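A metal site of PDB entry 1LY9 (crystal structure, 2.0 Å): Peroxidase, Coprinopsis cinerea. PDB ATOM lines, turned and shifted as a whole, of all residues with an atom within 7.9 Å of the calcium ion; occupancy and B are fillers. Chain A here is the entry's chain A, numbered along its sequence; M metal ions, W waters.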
ATOM      1  N   ILE A  52      26.840   8.068  24.940  1.00  0.00           N
ATOM      2  CA  ILE A  52      26.422   7.342  23.755  1.00  0.00           C
ATOM      3  C   ILE A  52      26.013   8.248  22.595  1.00  0.00           C
ATOM      4  O   ILE A  52      26.402   8.001  21.448  1.00  0.00           O
ATOM      5  CB  ILE A  52      25.243   6.388  24.069  1.00  0.00           C
ATOM      6  CG1 ILE A  52      25.738   5.254  24.985  1.00  0.00           C
ATOM      7  CG2 ILE A  52      24.655   5.822  22.779  1.00  0.00           C
ATOM      8  CD1 ILE A  52      24.665   4.256  25.380  1.00  0.00           C
ATOM      9  N   VAL A  53      25.221   9.290  22.866  1.00  0.00           N
ATOM     10  CA  VAL A  53      24.787  10.169  21.789  1.00  0.00           C
ATOM     11  C   VAL A  53      25.989  10.871  21.139  1.00  0.00           C
ATOM     12  O   VAL A  53      26.043  10.978  19.908  1.00  0.00           O
ATOM     13  CB  VAL A  53      23.754  11.223  22.281  1.00  0.00           C
ATOM     14  CG1 VAL A  53      24.393  12.239  23.232  1.00  0.00           C
ATOM     15  CG2 VAL A  53      23.119  11.930  21.075  1.00  0.00           C
ATOM     16  N   PHE A  54      26.942  11.307  21.957  1.00  0.00           N
ATOM     17  CA  PHE A  54      28.150  11.969  21.436  1.00  0.00           C
ATOM     18  C   PHE A  54      28.986  11.004  20.595  1.00  0.00           C
ATOM     19  O   PHE A  54      29.398  11.331  19.478  1.00  0.00           O
ATOM     20  CB  PHE A  54      29.005  12.488  22.607  1.00  0.00           C
ATOM     21  CG  PHE A  54      30.341  13.068  22.183  1.00  0.00           C
ATOM     22  CD1 PHE A  54      31.473  12.875  22.981  1.00  0.00           C
ATOM     23  CD2 PHE A  54      30.468  13.837  21.028  1.00  0.00           C
ATOM     24  CE1 PHE A  54      32.701  13.436  22.624  1.00  0.00           C
ATOM     25  CE2 PHE A  54      31.696  14.406  20.665  1.00  0.00           C
ATOM     26  CZ  PHE A  54      32.808  14.204  21.470  1.00  0.00           C
ATOM     27  N   HIS A  55      29.226   9.804  21.128  1.00  0.00           N
ATOM     28  CA  HIS A  55      30.029   8.803  20.425  1.00  0.00           C
ATOM     29  C   HIS A  55      29.390   8.276  19.158  1.00  0.00           C
ATOM     30  O   HIS A  55      30.095   7.868  18.237  1.00  0.00           O
ATOM     31  CB  HIS A  55      30.376   7.641  21.366  1.00  0.00           C
ATOM     32  CG  HIS A  55      31.293   8.025  22.486  1.00  0.00           C
ATOM     33  ND1 HIS A  55      31.869   7.096  23.335  1.00  0.00           N
ATOM     34  CD2 HIS A  55      31.733   9.241  22.903  1.00  0.00           C
ATOM     35  CE1 HIS A  55      32.618   7.723  24.225  1.00  0.00           C
ATOM     36  NE2 HIS A  55      32.557   9.028  23.985  1.00  0.00           N
ATOM     37  N   ASP A  56      28.067   8.257  19.110  1.00  0.00           N
ATOM     38  CA  ASP A  56      27.389   7.784  17.902  1.00  0.00           C
ATOM     39  C   ASP A  56      27.500   8.863  16.828  1.00  0.00           C
ATOM     40  O   ASP A  56      27.931   8.605  15.713  1.00  0.00           O
ATOM     41  CB  ASP A  56      25.908   7.511  18.198  1.00  0.00           C
ATOM     42  CG  ASP A  56      25.150   7.018  16.970  1.00  0.00           C
ATOM     43  OD1 ASP A  56      25.715   6.198  16.211  1.00  0.00           O
ATOM     44  OD2 ASP A  56      23.988   7.418  16.767  1.00  0.00           O
ATOM     45  N   ALA A  57      27.117  10.073  17.190  1.00  0.00           N
ATOM     46  CA  ALA A  57      27.113  11.198  16.270  1.00  0.00           C
ATOM     47  C   ALA A  57      28.478  11.625  15.723  1.00  0.00           C
ATOM     48  O   ALA A  57      28.598  11.954  14.549  1.00  0.00           O
ATOM     49  CB  ALA A  57      26.432  12.401  16.931  1.00  0.00           C
ATOM     50  N   ILE A  58      29.496  11.609  16.567  1.00  0.00           N
ATOM     51  CA  ILE A  58      30.816  12.050  16.160  1.00  0.00           C
ATOM     52  C   ILE A  58      31.532  11.149  15.147  1.00  0.00           C
ATOM     53  O   ILE A  58      32.568  11.526  14.594  1.00  0.00           O
ATOM     54  CB  ILE A  58      31.722  12.324  17.400  1.00  0.00           C
ATOM     55  CG1 ILE A  58      32.695  13.451  17.086  1.00  0.00           C
ATOM     56  CG2 ILE A  58      32.461  11.052  17.828  1.00  0.00           C
ATOM     57  CD1 ILE A  58      32.014  14.731  16.613  1.00  0.00           C
ATOM     58  N   GLY A  59      30.978   9.963  14.897  1.00  0.00           N
ATOM     59  CA  GLY A  59      31.576   9.060  13.925  1.00  0.00           C
ATOM     60  C   GLY A  59      31.102   9.550  12.566  1.00  0.00           C
ATOM     61  O   GLY A  59      30.262   8.922  11.916  1.00  0.00           O
ATOM     62  N   PHE A  60      31.640  10.686  12.166  1.00  0.00           N
ATOM     63  CA  PHE A  60      31.285  11.350  10.912  1.00  0.00           C
ATOM     64  C   PHE A  60      32.513  12.157  10.482  1.00  0.00           C
ATOM     65  O   PHE A  60      33.033  12.951  11.264  1.00  0.00           O
ATOM     66  CB  PHE A  60      30.095  12.285  11.158  1.00  0.00           C
ATOM     67  CG  PHE A  60      29.687  13.112   9.958  1.00  0.00           C
ATOM     68  CD1 PHE A  60      29.038  12.522   8.875  1.00  0.00           C
ATOM     69  CD2 PHE A  60      29.943  14.480   9.926  1.00  0.00           C
ATOM     70  CE1 PHE A  60      28.656  13.287   7.757  1.00  0.00           C
ATOM     71  CE2 PHE A  60      29.561  15.251   8.816  1.00  0.00           C
ATOM     72  CZ  PHE A  60      28.923  14.654   7.739  1.00  0.00           C
ATOM     73  N   GLY A  72      31.737   7.558   7.934  1.00  0.00           N
ATOM     74  CA  GLY A  72      30.769   7.303   8.995  1.00  0.00           C
ATOM     75  C   GLY A  72      29.463   8.013   8.700  1.00  0.00           C
ATOM     76  O   GLY A  72      29.461   9.034   8.008  1.00  0.00           O
ATOM     77  N   GLY A  73      28.359   7.490   9.213  1.00  0.00           N
ATOM     78  CA  GLY A  73      27.068   8.100   8.968  1.00  0.00           C
ATOM     79  C   GLY A  73      26.523   9.043  10.021  1.00  0.00           C
ATOM     80  O   GLY A  73      25.332   9.339  10.034  1.00  0.00           O
ATOM     81  N   GLY A  74      27.377   9.521  10.921  1.00  0.00           N
ATOM     82  CA  GLY A  74      26.901  10.442  11.940  1.00  0.00           C
ATOM     83  C   GLY A  74      25.963   9.827  12.969  1.00  0.00           C
ATOM     84  O   GLY A  74      26.220   8.751  13.498  1.00  0.00           O
ATOM     85  N   ALA A  75      24.862  10.529  13.264  1.00  0.00           N
ATOM     86  CA  ALA A  75      23.886  10.092  14.249  1.00  0.00           C
ATOM     87  C   ALA A  75      22.934   9.034  13.686  1.00  0.00           C
ATOM     88  O   ALA A  75      21.716   9.214  13.662  1.00  0.00           O
ATOM     89  CB  ALA A  75      23.089  11.299  14.759  1.00  0.00           C
ATOM     90  N   ASP A  76      23.511   7.924  13.258  1.00  0.00           N
ATOM     91  CA  ASP A  76      22.758   6.844  12.632  1.00  0.00           C
ATOM     92  C   ASP A  76      22.443   5.663  13.537  1.00  0.00           C
ATOM     93  O   ASP A  76      21.864   4.677  13.088  1.00  0.00           O
ATOM     94  CB  ASP A  76      23.542   6.359  11.418  1.00  0.00           C
ATOM     95  CG  ASP A  76      24.962   5.951  11.772  1.00  0.00           C
ATOM     96  OD1 ASP A  76      25.753   5.652  10.855  1.00  0.00           O
ATOM     97  OD2 ASP A  76      25.305   5.915  12.980  1.00  0.00           O
ATOM     98  N   GLY A  77      22.835   5.754  14.811  1.00  0.00           N
ATOM     99  CA  GLY A  77      22.568   4.657  15.740  1.00  0.00           C
ATOM    100  C   GLY A  77      23.488   3.467  15.528  1.00  0.00           C
ATOM    101  O   GLY A  77      23.255   2.389  16.079  1.00  0.00           O
ATOM    102  N   SER A  78      24.550   3.657  14.740  1.00  0.00           N
ATOM    103  CA  SER A  78      25.492   2.586  14.450  1.00  0.00           C
ATOM    104  C   SER A  78      26.115   1.967  15.691  1.00  0.00           C
ATOM    105  O   SER A  78      26.532   0.807  15.678  1.00  0.00           O
ATOM    106  CB  SER A  78      26.599   3.096  13.533  1.00  0.00           C
ATOM    107  OG  SER A  78      27.407   4.067  14.177  1.00  0.00           O
ATOM    108  N   ILE A  79      26.198   2.735  16.776  1.00  0.00           N
ATOM    109  CA  ILE A  79      26.786   2.258  18.010  1.00  0.00           C
ATOM    110  C   ILE A  79      25.955   1.117  18.595  1.00  0.00           C
ATOM    111  O   ILE A  79      26.464   0.292  19.354  1.00  0.00           O
ATOM    112  CB  ILE A  79      26.924   3.414  19.040  1.00  0.00           C
ATOM    113  CG1 ILE A  79      27.789   2.975  20.217  1.00  0.00           C
ATOM    114  CG2 ILE A  79      25.549   3.861  19.519  1.00  0.00           C
ATOM    115  CD1 ILE A  79      28.252   4.115  21.115  1.00  0.00           C
ATOM    116  N   ILE A  80      24.670   1.071  18.241  1.00  0.00           N
ATOM    117  CA  ILE A  80      23.771   0.024  18.707  1.00  0.00           C
ATOM    118  C   ILE A  80      23.682  -1.086  17.667  1.00  0.00           C
ATOM    119  O   ILE A  80      23.912  -2.262  17.982  1.00  0.00           O
ATOM    120  CB  ILE A  80      22.333   0.568  18.952  1.00  0.00           C
ATOM    121  CG1 ILE A  80      22.328   1.615  20.067  1.00  0.00           C
ATOM    122  CG2 ILE A  80      21.404  -0.596  19.331  1.00  0.00           C
ATOM    123  CD1 ILE A  80      20.947   2.236  20.327  1.00  0.00           C
ATOM    124  N   GLU A  86      31.679  -1.384  17.361  1.00  0.00           N
ATOM    125  CA  GLU A  86      31.901  -0.139  18.086  1.00  0.00           C
ATOM    126  C   GLU A  86      32.180  -0.261  19.585  1.00  0.00           C
ATOM    127  O   GLU A  86      32.980   0.510  20.129  1.00  0.00           O
ATOM    128  CB  GLU A  86      30.757   0.838  17.799  1.00  0.00           C
ATOM    129  CG  GLU A  86      30.722   1.234  16.327  1.00  0.00           C
ATOM    130  CD  GLU A  86      29.859   2.444  16.011  1.00  0.00           C
ATOM    131  OE1 GLU A  86      29.738   3.340  16.866  1.00  0.00           O
ATOM    132  OE2 GLU A  86      29.329   2.498  14.893  1.00  0.00           O
ATOM    133  N   GLY A 114      18.918   5.457  15.497  1.00  0.00           N
ATOM    134  CA  GLY A 114      19.411   6.821  15.389  1.00  0.00           C
ATOM    135  C   GLY A 114      18.431   7.745  16.103  1.00  0.00           C
ATOM    136  O   GLY A 114      18.839   8.599  16.892  1.00  0.00           O
ATOM    137  N   ILE A 117      18.274   7.077  20.134  1.00  0.00           N
ATOM    138  CA  ILE A 117      19.359   7.675  20.890  1.00  0.00           C
ATOM    139  C   ILE A 117      19.102   9.163  21.128  1.00  0.00           C
ATOM    140  O   ILE A 117      19.245   9.649  22.249  1.00  0.00           O
ATOM    141  CB  ILE A 117      20.716   7.478  20.161  1.00  0.00           C
ATOM    142  CG1 ILE A 117      21.126   6.000  20.225  1.00  0.00           C
ATOM    143  CG2 ILE A 117      21.807   8.358  20.793  1.00  0.00           C
ATOM    144  CD1 ILE A 117      22.407   5.678  19.504  1.00  0.00           C
ATOM    145  N   SER A 144      22.448   1.354   8.855  1.00  0.00           N
ATOM    146  CA  SER A 144      23.705   2.066   9.047  1.00  0.00           C
ATOM    147  C   SER A 144      24.908   1.157   8.869  1.00  0.00           C
ATOM    148  O   SER A 144      24.776  -0.068   8.865  1.00  0.00           O
ATOM    149  CB  SER A 144      23.757   2.657  10.466  1.00  0.00           C
ATOM    150  OG  SER A 144      23.891   1.622  11.428  1.00  0.00           O
ATOM    151  N   GLN A 145      26.074   1.778   8.730  1.00  0.00           N
ATOM    152  CA  GLN A 145      27.323   1.043   8.595  1.00  0.00           C
ATOM    153  C   GLN A 145      28.128   1.361   9.854  1.00  0.00           C
ATOM    154  O   GLN A 145      27.969   2.432  10.429  1.00  0.00           O
ATOM    155  CB  GLN A 145      28.087   1.490   7.357  1.00  0.00           C
ATOM    156  CG  GLN A 145      27.380   1.182   6.039  1.00  0.00           C
ATOM    157  CD  GLN A 145      28.284   1.363   4.835  1.00  0.00           C
ATOM    158  OE1 GLN A 145      28.789   2.464   4.574  1.00  0.00           O
ATOM    159  NE2 GLN A 145      28.507   0.288   4.099  1.00  0.00           N
ATOM    160  N   PRO A 146      28.977   0.439  10.305  1.00  0.00           N
ATOM    161  CA  PRO A 146      29.760   0.743  11.512  1.00  0.00           C
ATOM    162  C   PRO A 146      30.655   1.951  11.313  1.00  0.00           C
ATOM    163  O   PRO A 146      31.172   2.192  10.222  1.00  0.00           O
ATOM    164  CB  PRO A 146      30.543  -0.546  11.764  1.00  0.00           C
ATOM    165  CG  PRO A 146      30.653  -1.151  10.379  1.00  0.00           C
ATOM    166  CD  PRO A 146      29.289  -0.918   9.804  1.00  0.00           C
ATOM    167  N   SER A 147      30.827   2.725  12.380  1.00  0.00           N
ATOM    168  CA  SER A 147      31.669   3.910  12.338  1.00  0.00           C
ATOM    169  C   SER A 147      33.138   3.529  12.207  1.00  0.00           C
ATOM    170  O   SER A 147      33.582   2.502  12.719  1.00  0.00           O
ATOM    171  CB  SER A 147      31.468   4.729  13.615  1.00  0.00           C
ATOM    172  OG  SER A 147      32.530   5.644  13.845  1.00  0.00           O
ATOM    173  N   PRO A 148      33.912   4.346  11.479  1.00  0.00           N
ATOM    174  CA  PRO A 148      35.338   4.045  11.340  1.00  0.00           C
ATOM    175  C   PRO A 148      35.952   4.239  12.733  1.00  0.00           C
ATOM    176  O   PRO A 148      35.404   4.956  13.569  1.00  0.00           O
ATOM    177  CB  PRO A 148      35.823   5.111  10.368  1.00  0.00           C
ATOM    178  CG  PRO A 148      34.618   5.366   9.524  1.00  0.00           C
ATOM    179  CD  PRO A 148      33.508   5.407  10.540  1.00  0.00           C
ATOM    180  N   LEU A 282      24.010  15.224  12.220  1.00  0.00           N
ATOM    181  CA  LEU A 282      25.230  14.922  11.498  1.00  0.00           C
ATOM    182  C   LEU A 282      24.973  13.670  10.667  1.00  0.00           C
ATOM    183  O   LEU A 282      24.567  12.634  11.189  1.00  0.00           O
ATOM    184  CB  LEU A 282      26.401  14.664  12.457  1.00  0.00           C
ATOM    185  CG  LEU A 282      26.929  15.854  13.266  1.00  0.00           C
ATOM    186  CD1 LEU A 282      28.139  15.418  14.084  1.00  0.00           C
ATOM    187  CD2 LEU A 282      27.323  16.986  12.322  1.00  0.00           C
ATOM    188  N   PHE A 284      22.766  13.672   8.219  1.00  0.00           N
ATOM    189  CA  PHE A 284      21.381  13.761   7.753  1.00  0.00           C
ATOM    190  C   PHE A 284      21.008  15.185   7.330  1.00  0.00           C
ATOM    191  O   PHE A 284      21.731  16.136   7.603  1.00  0.00           O
ATOM    192  CB  PHE A 284      20.431  13.313   8.871  1.00  0.00           C
ATOM    193  CG  PHE A 284      20.615  11.872   9.287  1.00  0.00           C
ATOM    194  CD1 PHE A 284      19.948  10.849   8.629  1.00  0.00           C
ATOM    195  CD2 PHE A 284      21.461  11.549  10.338  1.00  0.00           C
ATOM    196  CE1 PHE A 284      20.106   9.525   9.020  1.00  0.00           C
ATOM    197  CE2 PHE A 284      21.630  10.224  10.742  1.00  0.00           C
ATOM    198  CZ  PHE A 284      20.952   9.208  10.079  1.00  0.00           C
HETATM  199 CA    CA M   1      27.062   6.665  14.334  1.00  0.00          CA
HETATM  200  O   HOH W   1      28.873   6.743  12.715  1.00  0.00           O
HETATM  201  O   HOH W   2      29.120   5.826  15.962  1.00  0.00           O
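N of Gly 74 sits at hydrogen-bond distance from O of Gly 59 (3.1 Å).
The side-chain carboxylate of Asp 56 is in hydrogen-bond range of the backbone NH of Gly 77 (2.8 Å).
The side-chain carboxylate of Glu 86 lies close to the side-chain hydroxyl of Ser 78, at 2.6 Å.
Within 4 Å of the calcium ion: Asp 56, Gly 74, Asp 76 and Ser 78.
The calcium ion is bound by OD2 of Asp 76 (2.3 Å), OD1 of Asp 56 (2.4 Å), O of Gly 74 (2.4 Å), water W1 (2.4 Å), O of Asp 56 (2.5 Å), OG of Ser 78 (2.6 Å) and water W2 (2.8 Å).
The calcium ion has seven donor atoms within binding distance.
Water W2 lies within hydrogen-bond range of OE1 of Glu 86 (2.7 Å) and O of His 55 (3.2 Å).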
